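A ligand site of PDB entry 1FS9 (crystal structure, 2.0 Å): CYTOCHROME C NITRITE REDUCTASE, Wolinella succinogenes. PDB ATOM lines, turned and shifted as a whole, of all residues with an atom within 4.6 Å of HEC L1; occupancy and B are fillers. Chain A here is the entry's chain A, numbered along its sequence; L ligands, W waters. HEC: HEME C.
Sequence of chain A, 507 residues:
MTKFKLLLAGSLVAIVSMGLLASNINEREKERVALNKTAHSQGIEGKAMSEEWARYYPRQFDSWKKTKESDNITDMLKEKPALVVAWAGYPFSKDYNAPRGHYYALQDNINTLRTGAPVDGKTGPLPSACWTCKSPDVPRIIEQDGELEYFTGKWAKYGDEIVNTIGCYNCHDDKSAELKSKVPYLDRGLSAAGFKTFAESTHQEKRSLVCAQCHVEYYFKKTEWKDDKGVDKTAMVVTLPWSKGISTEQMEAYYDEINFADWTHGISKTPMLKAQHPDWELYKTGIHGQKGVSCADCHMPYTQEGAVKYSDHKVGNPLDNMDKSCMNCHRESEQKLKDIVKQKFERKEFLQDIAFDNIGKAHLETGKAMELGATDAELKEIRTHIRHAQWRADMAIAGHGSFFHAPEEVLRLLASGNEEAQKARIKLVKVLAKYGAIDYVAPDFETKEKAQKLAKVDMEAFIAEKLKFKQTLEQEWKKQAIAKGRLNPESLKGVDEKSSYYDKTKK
Water W1 lies within hydrogen-bond range of the side-chain hydroxyl of Tyr 96 (2.6 Å), an oxygen (O2D) of HEC L1 (2.7 Å), the backbone carbonyl oxygen of Ala 398 (2.7 Å) and a ring nitrogen (NE2) of His 400 (3.2 Å).
Water W6 lies within hydrogen-bond range of O1A of HEC L1 (2.7 Å) and OD1 of Asn 97 (3.1 Å).
Water W4 lies within hydrogen-bond range of O2D of HEC L1 (2.8 Å), OD1 of Asp 279 (2.8 Å) and N of His 400 (3.0 Å).
Water W5 lies within hydrogen-bond range of OG1 of Thr 112 (2.8 Å), O1A of HEC L1 (2.8 Å), NH1 of Arg 114 (3.3 Å), N of Tyr 96 (3.4 Å) and OD1 of Asn 97 (3.4 Å).
Water W8 lies within hydrogen-bond range of the backbone carbonyl oxygen of Asn 97 (2.8 Å), a ring nitrogen (NE2) of His 400 (2.9 Å), an oxygen (O1D) of HEC L1 (2.9 Å) and the side-chain hydroxyl of Tyr 96 (3.4 Å).
A ring nitrogen (NE2) of His 400 lies within hydrogen-bond range of the side-chain hydroxyl of Tyr 96.
OD2 of Asp 279 lies within hydrogen-bond range of ND1 of His 215.
O of Cys 130 is in hydrogen-bond range of ND2 of Asn 109 (3.1 Å).
The backbone carbonyl oxygen (O) of Val 216 lies within hydrogen-bond range of a ring nitrogen (ND1) of His 277.
The side-chain hydroxyl (OH) of Tyr 185 sits at hydrogen-bond distance from the backbone carbonyl oxygen (O) of Gln 213 (2.6 Å).
SG of Cys 133 lies within hydrogen-bond range of OH of Tyr 185.
O of Thr 112 is in hydrogen-bond range of OG1 of Thr 115 (3.0 Å).
O of Asn 109 sits at hydrogen-bond distance from OG1 of Thr 115 (3.1 Å).
An iron atom (FE) of HEC L1 is bound by the side-chain amino group (NZ) of Lys 134.
SG of Cys 214 is covalently linked to CAC of HEC L2, 1.8 Å away.
SG of Cys 130 is bonded to CAB of HEC L1.
A carbon (CAC) of HEC L1 is covalently linked to the side-chain sulfur of Cys 133, at 1.8 Å.
A ring nitrogen (NE2) of His 215 binds an iron atom (FE) of HEC L2.
OD2 of Asp 108 sits close to O2D of HEC L2, at 2.5 Å.
O2A of HEC L1 lies within salt-bridge range of NH1 of Arg 114 (3.0 Å).
The backbone NH (N) of Asn 97 is in hydrogen-bond range of an oxygen (O1A) of HEC L1 (3.0 Å).
A ring nitrogen (NE2) of His 277 sits close to a nitrogen (ND) of HEC L1.
Merely in contact with HEC L1: Tyr 96, Pro 99, Asp 108, Asn 109, Thr 112, Thr 115, Leu 126, Tyr 185, Gln 213, Cys 214, His 215, Tyr 218, Phe 220, Val 238, Ala 398 and His 400.
Of the 27 residues printed, 22 come within 4 Å of HEC L1.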
ATOM      1  N   TYR A  96      19.741 -10.876  31.651  1.00  0.00           N
ATOM      2  CA  TYR A  96      19.205 -11.949  30.802  1.00  0.00           C
ATOM      3  C   TYR A  96      17.720 -11.695  30.589  1.00  0.00           C
ATOM      4  O   TYR A  96      16.928 -11.796  31.523  1.00  0.00           O
ATOM      5  CB  TYR A  96      19.404 -13.327  31.459  1.00  0.00           C
ATOM      6  CG  TYR A  96      18.703 -14.450  30.716  1.00  0.00           C
ATOM      7  CD1 TYR A  96      19.002 -14.719  29.373  1.00  0.00           C
ATOM      8  CD2 TYR A  96      17.735 -15.229  31.347  1.00  0.00           C
ATOM      9  CE1 TYR A  96      18.328 -15.738  28.676  1.00  0.00           C
ATOM     10  CE2 TYR A  96      17.061 -16.247  30.649  1.00  0.00           C
ATOM     11  CZ  TYR A  96      17.366 -16.495  29.327  1.00  0.00           C
ATOM     12  OH  TYR A  96      16.688 -17.485  28.645  1.00  0.00           O
ATOM     13  N   ASN A  97      17.360 -11.331  29.352  1.00  0.00           N
ATOM     14  CA  ASN A  97      15.984 -11.038  28.997  1.00  0.00           C
ATOM     15  C   ASN A  97      15.451 -12.027  27.975  1.00  0.00           C
ATOM     16  O   ASN A  97      16.229 -12.682  27.277  1.00  0.00           O
ATOM     17  CB  ASN A  97      15.891  -9.632  28.418  1.00  0.00           C
ATOM     18  CG  ASN A  97      16.568  -8.598  29.287  1.00  0.00           C
ATOM     19  OD1 ASN A  97      17.369  -7.784  28.802  1.00  0.00           O
ATOM     20  ND2 ASN A  97      16.263  -8.612  30.577  1.00  0.00           N
ATOM     21  N   ALA A  98      14.125 -12.139  27.888  1.00  0.00           N
ATOM     22  CA  ALA A  98      13.512 -13.044  26.928  1.00  0.00           C
ATOM     23  C   ALA A  98      13.752 -12.451  25.546  1.00  0.00           C
ATOM     24  O   ALA A  98      14.051 -11.269  25.414  1.00  0.00           O
ATOM     25  CB  ALA A  98      12.015 -13.168  27.195  1.00  0.00           C
ATOM     26  N   PRO A  99      13.636 -13.267  24.495  1.00  0.00           N
ATOM     27  CA  PRO A  99      13.867 -12.730  23.163  1.00  0.00           C
ATOM     28  C   PRO A  99      12.722 -11.874  22.646  1.00  0.00           C
ATOM     29  O   PRO A  99      11.575 -12.080  23.018  1.00  0.00           O
ATOM     30  CB  PRO A  99      14.079 -13.980  22.311  1.00  0.00           C
ATOM     31  CG  PRO A  99      13.184 -14.984  22.972  1.00  0.00           C
ATOM     32  CD  PRO A  99      13.395 -14.732  24.445  1.00  0.00           C
ATOM     33  N   ASP A 108      20.232  -5.136  21.211  1.00  0.00           N
ATOM     34  CA  ASP A 108      20.189  -5.844  22.497  1.00  0.00           C
ATOM     35  C   ASP A 108      21.558  -6.450  22.800  1.00  0.00           C
ATOM     36  O   ASP A 108      21.962  -6.534  23.962  1.00  0.00           O
ATOM     37  CB  ASP A 108      19.103  -6.924  22.479  1.00  0.00           C
ATOM     38  CG  ASP A 108      17.701  -6.348  22.530  1.00  0.00           C
ATOM     39  OD1 ASP A 108      17.572  -5.165  22.915  1.00  0.00           O
ATOM     40  OD2 ASP A 108      16.735  -7.058  22.188  1.00  0.00           O
ATOM     41  N   ASN A 109      22.264  -6.847  21.747  1.00  0.00           N
ATOM     42  CA  ASN A 109      23.610  -7.410  21.891  1.00  0.00           C
ATOM     43  C   ASN A 109      24.477  -6.315  22.502  1.00  0.00           C
ATOM     44  O   ASN A 109      25.337  -6.579  23.346  1.00  0.00           O
ATOM     45  CB  ASN A 109      24.135  -7.803  20.516  1.00  0.00           C
ATOM     46  CG  ASN A 109      25.498  -8.467  20.565  1.00  0.00           C
ATOM     47  OD1 ASN A 109      26.478  -7.923  20.059  1.00  0.00           O
ATOM     48  ND2 ASN A 109      25.564  -9.637  21.192  1.00  0.00           N
ATOM     49  N   THR A 112      22.840  -5.317  26.436  1.00  0.00           N
ATOM     50  CA  THR A 112      22.958  -6.259  27.539  1.00  0.00           C
ATOM     51  C   THR A 112      24.178  -5.983  28.388  1.00  0.00           C
ATOM     52  O   THR A 112      25.259  -5.645  27.885  1.00  0.00           O
ATOM     53  CB  THR A 112      22.994  -7.727  27.048  1.00  0.00           C
ATOM     54  OG1 THR A 112      23.033  -8.599  28.188  1.00  0.00           O
ATOM     55  CG2 THR A 112      24.217  -7.992  26.185  1.00  0.00           C
ATOM     56  N   ARG A 114      25.840  -8.042  29.742  1.00  0.00           N
ATOM     57  CA  ARG A 114      26.790  -9.116  29.508  1.00  0.00           C
ATOM     58  C   ARG A 114      27.989  -8.670  28.674  1.00  0.00           C
ATOM     59  O   ARG A 114      29.101  -9.150  28.899  1.00  0.00           O
ATOM     60  CB  ARG A 114      26.106 -10.318  28.846  1.00  0.00           C
ATOM     61  CG  ARG A 114      24.925 -10.880  29.643  1.00  0.00           C
ATOM     62  CD  ARG A 114      24.719 -12.384  29.419  1.00  0.00           C
ATOM     63  NE  ARG A 114      24.317 -12.734  28.055  1.00  0.00           N
ATOM     64  CZ  ARG A 114      23.083 -12.623  27.575  1.00  0.00           C
ATOM     65  NH1 ARG A 114      22.104 -12.151  28.348  1.00  0.00           N
ATOM     66  NH2 ARG A 114      22.819 -12.997  26.337  1.00  0.00           N
ATOM     67  N   THR A 115      27.792  -7.763  27.721  1.00  0.00           N
ATOM     68  CA  THR A 115      28.898  -7.295  26.894  1.00  0.00           C
ATOM     69  C   THR A 115      29.734  -6.218  27.580  1.00  0.00           C
ATOM     70  O   THR A 115      30.774  -5.813  27.068  1.00  0.00           O
ATOM     71  CB  THR A 115      28.424  -6.774  25.509  1.00  0.00           C
ATOM     72  OG1 THR A 115      27.302  -5.892  25.687  1.00  0.00           O
ATOM     73  CG2 THR A 115      28.030  -7.944  24.609  1.00  0.00           C
ATOM     74  N   LEU A 126      33.669  -9.690  26.675  1.00  0.00           N
ATOM     75  CA  LEU A 126      33.410 -10.729  25.677  1.00  0.00           C
ATOM     76  C   LEU A 126      34.166 -10.629  24.347  1.00  0.00           C
ATOM     77  O   LEU A 126      34.636  -9.548  23.960  1.00  0.00           O
ATOM     78  CB  LEU A 126      31.904 -10.801  25.419  1.00  0.00           C
ATOM     79  CG  LEU A 126      31.065 -10.987  26.690  1.00  0.00           C
ATOM     80  CD1 LEU A 126      29.588 -11.097  26.332  1.00  0.00           C
ATOM     81  CD2 LEU A 126      31.528 -12.236  27.429  1.00  0.00           C
ATOM     82  N   ALA A 129      33.014 -13.265  18.762  1.00  0.00           N
ATOM     83  CA  ALA A 129      31.999 -14.247  18.416  1.00  0.00           C
ATOM     84  C   ALA A 129      30.586 -13.844  18.850  1.00  0.00           C
ATOM     85  O   ALA A 129      29.611 -14.391  18.345  1.00  0.00           O
ATOM     86  CB  ALA A 129      32.363 -15.610  18.988  1.00  0.00           C
ATOM     87  N   CYS A 130      30.473 -12.898  19.772  1.00  0.00           N
ATOM     88  CA  CYS A 130      29.145 -12.494  20.226  1.00  0.00           C
ATOM     89  C   CYS A 130      28.314 -11.759  19.185  1.00  0.00           C
ATOM     90  O   CYS A 130      27.120 -11.574  19.379  1.00  0.00           O
ATOM     91  CB  CYS A 130      29.250 -11.647  21.505  1.00  0.00           C
ATOM     92  SG  CYS A 130      29.587 -12.631  22.987  1.00  0.00           S
ATOM     93  N   THR A 132      28.307 -12.796  15.873  1.00  0.00           N
ATOM     94  CA  THR A 132      27.949 -13.883  14.966  1.00  0.00           C
ATOM     95  C   THR A 132      26.488 -14.065  14.562  1.00  0.00           C
ATOM     96  O   THR A 132      26.170 -14.094  13.379  1.00  0.00           O
ATOM     97  CB  THR A 132      28.469 -15.223  15.507  1.00  0.00           C
ATOM     98  OG1 THR A 132      29.833 -15.075  15.920  1.00  0.00           O
ATOM     99  CG2 THR A 132      28.394 -16.298  14.423  1.00  0.00           C
ATOM    100  N   CYS A 133      25.604 -14.187  15.537  1.00  0.00           N
ATOM    101  CA  CYS A 133      24.194 -14.422  15.240  1.00  0.00           C
ATOM    102  C   CYS A 133      23.324 -13.198  15.421  1.00  0.00           C
ATOM    103  O   CYS A 133      22.142 -13.317  15.748  1.00  0.00           O
ATOM    104  CB  CYS A 133      23.689 -15.560  16.120  1.00  0.00           C
ATOM    105  SG  CYS A 133      24.731 -17.037  16.072  1.00  0.00           S
ATOM    106  N   LYS A 134      23.877 -12.016  15.175  1.00  0.00           N
ATOM    107  CA  LYS A 134      23.128 -10.786  15.367  1.00  0.00           C
ATOM    108  C   LYS A 134      23.100  -9.859  14.154  1.00  0.00           C
ATOM    109  O   LYS A 134      22.350  -8.880  14.140  1.00  0.00           O
ATOM    110  CB  LYS A 134      23.732 -10.007  16.525  1.00  0.00           C
ATOM    111  CG  LYS A 134      23.805 -10.752  17.846  1.00  0.00           C
ATOM    112  CD  LYS A 134      22.403 -10.951  18.426  1.00  0.00           C
ATOM    113  CE  LYS A 134      22.460 -11.624  19.794  1.00  0.00           C
ATOM    114  NZ  LYS A 134      23.023 -13.001  19.740  1.00  0.00           N
ATOM    115  N   TYR A 185      30.090 -23.078  10.711  1.00  0.00           N
ATOM    116  CA  TYR A 185      29.953 -23.943  11.872  1.00  0.00           C
ATOM    117  C   TYR A 185      28.686 -24.818  11.839  1.00  0.00           C
ATOM    118  O   TYR A 185      28.670 -25.890  12.436  1.00  0.00           O
ATOM    119  CB  TYR A 185      30.024 -23.129  13.169  1.00  0.00           C
ATOM    120  CG  TYR A 185      28.970 -22.046  13.337  1.00  0.00           C
ATOM    121  CD1 TYR A 185      27.639 -22.375  13.593  1.00  0.00           C
ATOM    122  CD2 TYR A 185      29.317 -20.698  13.263  1.00  0.00           C
ATOM    123  CE1 TYR A 185      26.669 -21.384  13.777  1.00  0.00           C
ATOM    124  CE2 TYR A 185      28.354 -19.693  13.456  1.00  0.00           C
ATOM    125  CZ  TYR A 185      27.038 -20.051  13.714  1.00  0.00           C
ATOM    126  OH  TYR A 185      26.077 -19.075  13.916  1.00  0.00           O
ATOM    127  N   GLN A 213      21.082 -21.582  12.017  1.00  0.00           N
ATOM    128  CA  GLN A 213      22.378 -20.922  11.990  1.00  0.00           C
ATOM    129  C   GLN A 213      22.582 -20.231  13.332  1.00  0.00           C
ATOM    130  O   GLN A 213      23.712 -20.114  13.812  1.00  0.00           O
ATOM    131  CB  GLN A 213      22.426 -19.822  10.924  1.00  0.00           C
ATOM    132  CG  GLN A 213      22.110 -20.236   9.518  1.00  0.00           C
ATOM    133  CD  GLN A 213      22.181 -19.051   8.592  1.00  0.00           C
ATOM    134  OE1 GLN A 213      23.264 -18.592   8.231  1.00  0.00           O
ATOM    135  NE2 GLN A 213      21.015 -18.519   8.226  1.00  0.00           N
ATOM    136  N   CYS A 214      21.495 -19.773  13.937  1.00  0.00           N
ATOM    137  CA  CYS A 214      21.579 -19.066  15.200  1.00  0.00           C
ATOM    138  C   CYS A 214      20.831 -19.686  16.379  1.00  0.00           C
ATOM    139  O   CYS A 214      21.313 -19.642  17.501  1.00  0.00           O
ATOM    140  CB  CYS A 214      21.077 -17.625  15.011  1.00  0.00           C
ATOM    141  SG  CYS A 214      21.778 -16.763  13.579  1.00  0.00           S
ATOM    142  N   HIS A 215      19.667 -20.252  16.100  1.00  0.00           N
ATOM    143  CA  HIS A 215      18.835 -20.845  17.145  1.00  0.00           C
ATOM    144  C   HIS A 215      19.268 -22.244  17.560  1.00  0.00           C
ATOM    145  O   HIS A 215      18.507 -23.215  17.448  1.00  0.00           O
ATOM    146  CB  HIS A 215      17.375 -20.844  16.688  1.00  0.00           C
ATOM    147  CG  HIS A 215      16.727 -19.496  16.755  1.00  0.00           C
ATOM    148  ND1 HIS A 215      16.080 -19.011  17.881  1.00  0.00           N
ATOM    149  CD2 HIS A 215      16.673 -18.493  15.850  1.00  0.00           C
ATOM    150  CE1 HIS A 215      15.663 -17.761  17.612  1.00  0.00           C
ATOM    151  NE2 HIS A 215      16.006 -17.402  16.382  1.00  0.00           N
ATOM    152  N   VAL A 216      20.498 -22.333  18.043  1.00  0.00           N
ATOM    153  CA  VAL A 216      21.078 -23.608  18.481  1.00  0.00           C
ATOM    154  C   VAL A 216      22.004 -23.377  19.676  1.00  0.00           C
ATOM    155  O   VAL A 216      22.403 -22.242  19.946  1.00  0.00           O
ATOM    156  CB  VAL A 216      21.918 -24.243  17.354  1.00  0.00           C
ATOM    157  CG1 VAL A 216      21.021 -24.617  16.173  1.00  0.00           C
ATOM    158  CG2 VAL A 216      23.011 -23.267  16.924  1.00  0.00           C
ATOM    159  N   TYR A 218      25.598 -23.791  21.628  1.00  0.00           N
ATOM    160  CA  TYR A 218      26.970 -23.723  21.142  1.00  0.00           C
ATOM    161  C   TYR A 218      27.941 -23.419  22.277  1.00  0.00           C
ATOM    162  O   TYR A 218      27.534 -23.129  23.406  1.00  0.00           O
ATOM    163  CB  TYR A 218      27.109 -22.601  20.116  1.00  0.00           C
ATOM    164  CG  TYR A 218      27.079 -21.238  20.784  1.00  0.00           C
ATOM    165  CD1 TYR A 218      25.878 -20.660  21.206  1.00  0.00           C
ATOM    166  CD2 TYR A 218      28.273 -20.596  21.118  1.00  0.00           C
ATOM    167  CE1 TYR A 218      25.874 -19.476  21.957  1.00  0.00           C
ATOM    168  CE2 TYR A 218      28.279 -19.420  21.875  1.00  0.00           C
ATOM    169  CZ  TYR A 218      27.081 -18.878  22.293  1.00  0.00           C
ATOM    170  OH  TYR A 218      27.106 -17.738  23.072  1.00  0.00           O
ATOM    171  N   PHE A 220      32.313 -21.771  22.760  1.00  0.00           N
ATOM    172  CA  PHE A 220      33.443 -21.161  22.064  1.00  0.00           C
ATOM    173  C   PHE A 220      34.662 -22.055  22.235  1.00  0.00           C
ATOM    174  O   PHE A 220      35.091 -22.326  23.354  1.00  0.00           O
ATOM    175  CB  PHE A 220      33.772 -19.770  22.640  1.00  0.00           C
ATOM    176  CG  PHE A 220      32.680 -18.759  22.445  1.00  0.00           C
ATOM    177  CD1 PHE A 220      31.929 -18.726  21.274  1.00  0.00           C
ATOM    178  CD2 PHE A 220      32.442 -17.796  23.418  1.00  0.00           C
ATOM    179  CE1 PHE A 220      30.945 -17.752  21.073  1.00  0.00           C
ATOM    180  CE2 PHE A 220      31.464 -16.808  23.225  1.00  0.00           C
ATOM    181  CZ  PHE A 220      30.712 -16.789  22.054  1.00  0.00           C
ATOM    182  N   VAL A 238      32.858 -20.322  17.338  1.00  0.00           N
ATOM    183  CA  VAL A 238      31.530 -20.835  17.655  1.00  0.00           C
ATOM    184  C   VAL A 238      31.503 -22.277  17.179  1.00  0.00           C
ATOM    185  O   VAL A 238      31.791 -22.558  16.015  1.00  0.00           O
ATOM    186  CB  VAL A 238      30.422 -20.047  16.917  1.00  0.00           C
ATOM    187  CG1 VAL A 238      29.065 -20.736  17.082  1.00  0.00           C
ATOM    188  CG2 VAL A 238      30.350 -18.626  17.450  1.00  0.00           C
ATOM    189  N   HIS A 277      19.761 -21.208  24.122  1.00  0.00           N
ATOM    190  CA  HIS A 277      18.691 -21.397  23.152  1.00  0.00           C
ATOM    191  C   HIS A 277      18.857 -22.553  22.168  1.00  0.00           C
ATOM    192  O   HIS A 277      19.115 -22.343  20.982  1.00  0.00           O
ATOM    193  CB  HIS A 277      18.544 -20.095  22.370  1.00  0.00           C
ATOM    194  CG  HIS A 277      19.840 -19.467  21.983  1.00  0.00           C
ATOM    195  ND1 HIS A 277      20.758 -20.105  21.157  1.00  0.00           N
ATOM    196  CD2 HIS A 277      20.424 -18.303  22.367  1.00  0.00           C
ATOM    197  CE1 HIS A 277      21.841 -19.353  21.050  1.00  0.00           C
ATOM    198  NE2 HIS A 277      21.664 -18.254  21.771  1.00  0.00           N
ATOM    199  N   ASP A 279      16.983 -24.127  20.484  1.00  0.00           N
ATOM    200  CA  ASP A 279      15.675 -24.182  19.844  1.00  0.00           C
ATOM    201  C   ASP A 279      15.542 -25.287  18.793  1.00  0.00           C
ATOM    202  O   ASP A 279      14.596 -26.080  18.831  1.00  0.00           O
ATOM    203  CB  ASP A 279      15.326 -22.834  19.216  1.00  0.00           C
ATOM    204  CG  ASP A 279      15.506 -21.662  20.172  1.00  0.00           C
ATOM    205  OD1 ASP A 279      14.904 -21.684  21.264  1.00  0.00           O
ATOM    206  OD2 ASP A 279      16.246 -20.722  19.831  1.00  0.00           O
ATOM    207  N   ALA A 398      16.229 -23.035  28.205  1.00  0.00           N
ATOM    208  CA  ALA A 398      16.933 -22.018  27.413  1.00  0.00           C
ATOM    209  C   ALA A 398      16.244 -21.736  26.088  1.00  0.00           C
ATOM    210  O   ALA A 398      16.386 -20.653  25.522  1.00  0.00           O
ATOM    211  CB  ALA A 398      18.379 -22.443  27.191  1.00  0.00           C
ATOM    212  N   HIS A 400      13.071 -20.853  24.705  1.00  0.00           N
ATOM    213  CA  HIS A 400      11.784 -20.339  25.185  1.00  0.00           C
ATOM    214  C   HIS A 400      10.533 -20.937  24.551  1.00  0.00           C
ATOM    215  O   HIS A 400       9.447 -20.827  25.108  1.00  0.00           O
ATOM    216  CB  HIS A 400      11.757 -18.813  25.024  1.00  0.00           C
ATOM    217  CG  HIS A 400      12.683 -18.103  25.957  1.00  0.00           C
ATOM    218  ND1 HIS A 400      12.326 -17.745  27.244  1.00  0.00           N
ATOM    219  CD2 HIS A 400      13.976 -17.707  25.807  1.00  0.00           C
ATOM    220  CE1 HIS A 400      13.358 -17.173  27.844  1.00  0.00           C
ATOM    221  NE2 HIS A 400      14.364 -17.137  26.991  1.00  0.00           N
HETATM  222 FE   HEC L   1      22.898 -14.316  21.516  1.00  0.00          FE
HETATM  223  CHA HEC L   1      19.590 -13.661  22.035  1.00  0.00           C
HETATM  224  CHB HEC L   1      23.753 -11.691  23.405  1.00  0.00           C
HETATM  225  CHC HEC L   1      26.168 -15.250  21.253  1.00  0.00           C
HETATM  226  CHD HEC L   1      22.040 -16.541  19.134  1.00  0.00           C
HETATM  227  NA  HEC L   1      21.877 -12.938  22.498  1.00  0.00           N
HETATM  228  C1A HEC L   1      20.514 -12.783  22.604  1.00  0.00           C
HETATM  229  C2A HEC L   1      20.157 -11.607  23.387  1.00  0.00           C
HETATM  230  C3A HEC L   1      21.330 -11.041  23.765  1.00  0.00           C
HETATM  231  C4A HEC L   1      22.383 -11.878  23.213  1.00  0.00           C
HETATM  232  CMA HEC L   1      21.489  -9.811  24.678  1.00  0.00           C
HETATM  233  CAA HEC L   1      18.752 -11.148  23.772  1.00  0.00           C
HETATM  234  CBA HEC L   1      18.211 -11.990  24.928  1.00  0.00           C
HETATM  235  CGA HEC L   1      19.004 -11.791  26.209  1.00  0.00           C
HETATM  236  O1A HEC L   1      18.849 -10.731  26.848  1.00  0.00           O
HETATM  237  O2A HEC L   1      19.781 -12.691  26.581  1.00  0.00           O
HETATM  238  NB  HEC L   1      24.594 -13.624  22.195  1.00  0.00           N
HETATM  239  C1B HEC L   1      24.774 -12.503  22.976  1.00  0.00           C
HETATM  240  C2B HEC L   1      26.142 -12.405  23.444  1.00  0.00           C
HETATM  241  C3B HEC L   1      26.823 -13.448  22.916  1.00  0.00           C
HETATM  242  C4B HEC L   1      25.860 -14.190  22.107  1.00  0.00           C
HETATM  243  CMB HEC L   1      26.669 -11.401  24.481  1.00  0.00           C
HETATM  244  CAB HEC L   1      28.161 -13.761  23.166  1.00  0.00           C
HETATM  245  CBB HEC L   1      28.486 -14.642  24.207  1.00  0.00           C
HETATM  246  NC  HEC L   1      23.896 -15.636  20.434  1.00  0.00           N
HETATM  247  C1C HEC L   1      25.247 -15.917  20.434  1.00  0.00           C
HETATM  248  C2C HEC L   1      25.602 -16.868  19.394  1.00  0.00           C
HETATM  249  C3C HEC L   1      24.449 -17.176  18.747  1.00  0.00           C
HETATM  250  C4C HEC L   1      23.393 -16.443  19.436  1.00  0.00           C
HETATM  251  CMC HEC L   1      27.004 -17.390  19.054  1.00  0.00           C
HETATM  252  CAC HEC L   1      24.309 -17.963  17.596  1.00  0.00           C
HETATM  253  CBC HEC L   1      24.879 -19.256  17.460  1.00  0.00           C
HETATM  254  ND  HEC L   1      21.188 -15.028  20.832  1.00  0.00           N
HETATM  255  C1D HEC L   1      21.002 -15.924  19.785  1.00  0.00           C
HETATM  256  C2D HEC L   1      19.604 -16.293  19.627  1.00  0.00           C
HETATM  257  C3D HEC L   1      18.914 -15.594  20.565  1.00  0.00           C
HETATM  258  C4D HEC L   1      19.910 -14.763  21.264  1.00  0.00           C
HETATM  259  CMD HEC L   1      19.000 -17.277  18.623  1.00  0.00           C
HETATM  260  CAD HEC L   1      17.395 -15.582  20.734  1.00  0.00           C
HETATM  261  CBD HEC L   1      16.696 -16.706  21.508  1.00  0.00           C
HETATM  262  CGD HEC L   1      16.961 -16.649  23.000  1.00  0.00           C
HETATM  263  O1D HEC L   1      17.523 -15.652  23.484  1.00  0.00           O
HETATM  264  O2D HEC L   1      16.577 -17.613  23.700  1.00  0.00           O
HETATM  265 FE   HEC L   2      15.529 -15.622  15.392  1.00  0.00          FE
HETATM  266  CHA HEC L   2      14.598 -13.866  18.153  1.00  0.00           C
HETATM  267  CHB HEC L   2      12.563 -17.148  15.297  1.00  0.00           C
HETATM  268  CHC HEC L   2      16.304 -16.957  12.389  1.00  0.00           C
HETATM  269  CHD HEC L   2      18.704 -14.564  15.765  1.00  0.00           C
HETATM  270  NA  HEC L   2      13.911 -15.467  16.435  1.00  0.00           N
HETATM  271  C1A HEC L   2      13.647 -14.643  17.523  1.00  0.00           C
HETATM  272  C2A HEC L   2      12.300 -14.848  18.001  1.00  0.00           C
HETATM  273  C3A HEC L   2      11.757 -15.827  17.228  1.00  0.00           C
HETATM  274  C4A HEC L   2      12.758 -16.203  16.283  1.00  0.00           C
HETATM  275  CMA HEC L   2      10.334 -16.377  17.275  1.00  0.00           C
HETATM  276  CAA HEC L   2      11.591 -14.060  19.092  1.00  0.00           C
HETATM  277  CBA HEC L   2      10.538 -13.141  18.500  1.00  0.00           C
HETATM  278  CGA HEC L   2       9.830 -12.297  19.558  1.00  0.00           C
HETATM  279  O1A HEC L   2       9.963 -12.615  20.766  1.00  0.00           O
HETATM  280  O2A HEC L   2       9.151 -11.326  19.190  1.00  0.00           O
HETATM  281  NB  HEC L   2      14.613 -16.826  14.111  1.00  0.00           N
HETATM  282  C1B HEC L   2      13.393 -17.419  14.258  1.00  0.00           C
HETATM  283  C2B HEC L   2      13.065 -18.276  13.133  1.00  0.00           C
HETATM  284  C3B HEC L   2      14.070 -18.156  12.237  1.00  0.00           C
HETATM  285  C4B HEC L   2      15.053 -17.268  12.877  1.00  0.00           C
HETATM  286  CMB HEC L   2      11.839 -19.176  13.018  1.00  0.00           C
HETATM  287  CAB HEC L   2      14.129 -18.753  10.965  1.00  0.00           C
HETATM  288  CBB HEC L   2      13.142 -18.510   9.963  1.00  0.00           C
HETATM  289  NC  HEC L   2      17.153 -15.707  14.290  1.00  0.00           N
HETATM  290  C1C HEC L   2      17.291 -16.239  13.032  1.00  0.00           C
HETATM  291  C2C HEC L   2      18.639 -16.099  12.550  1.00  0.00           C
HETATM  292  C3C HEC L   2      19.356 -15.485  13.532  1.00  0.00           C
HETATM  293  C4C HEC L   2      18.415 -15.255  14.600  1.00  0.00           C
HETATM  294  CMC HEC L   2      19.197 -16.622  11.221  1.00  0.00           C
HETATM  295  CAC HEC L   2      20.741 -15.244  13.520  1.00  0.00           C
HETATM  296  CBC HEC L   2      21.369 -14.493  12.496  1.00  0.00           C
HETATM  297  ND  HEC L   2      16.473 -14.519  16.734  1.00  0.00           N
HETATM  298  C1D HEC L   2      17.817 -14.197  16.737  1.00  0.00           C
HETATM  299  C2D HEC L   2      18.120 -13.267  17.810  1.00  0.00           C
HETATM  300  C3D HEC L   2      16.979 -13.053  18.483  1.00  0.00           C
HETATM  301  C4D HEC L   2      15.944 -13.831  17.809  1.00  0.00           C
HETATM  302  CMD HEC L   2      19.504 -12.745  18.190  1.00  0.00           C
HETATM  303  CAD HEC L   2      16.844 -12.194  19.729  1.00  0.00           C
HETATM  304  CBD HEC L   2      16.348 -10.805  19.349  1.00  0.00           C
HETATM  305  CGD HEC L   2      16.348  -9.844  20.531  1.00  0.00           C
HETATM  306  O1D HEC L   2      15.838 -10.214  21.604  1.00  0.00           O
HETATM  307  O2D HEC L   2      16.850  -8.707  20.359  1.00  0.00           O
HETATM  308  O   HOH W   1      17.326 -18.215  26.207  1.00  0.00           O
HETATM  309  O   HOH W   2      22.948 -15.410  23.267  1.00  0.00           O
HETATM  310  O   HOH W   3      25.663 -13.598  18.467  1.00  0.00           O
HETATM  311  O   HOH W   4      14.578 -19.263  22.723  1.00  0.00           O
HETATM  312  O   HOH W   5      20.410  -9.316  28.721  1.00  0.00           O
HETATM  313  O   HOH W   6      17.953  -8.402  25.809  1.00  0.00           O
HETATM  314  O   HOH W   7      19.713 -15.278  25.369  1.00  0.00           O
HETATM  315  O   HOH W   8      16.316 -15.260  26.091  1.00  0.00           O
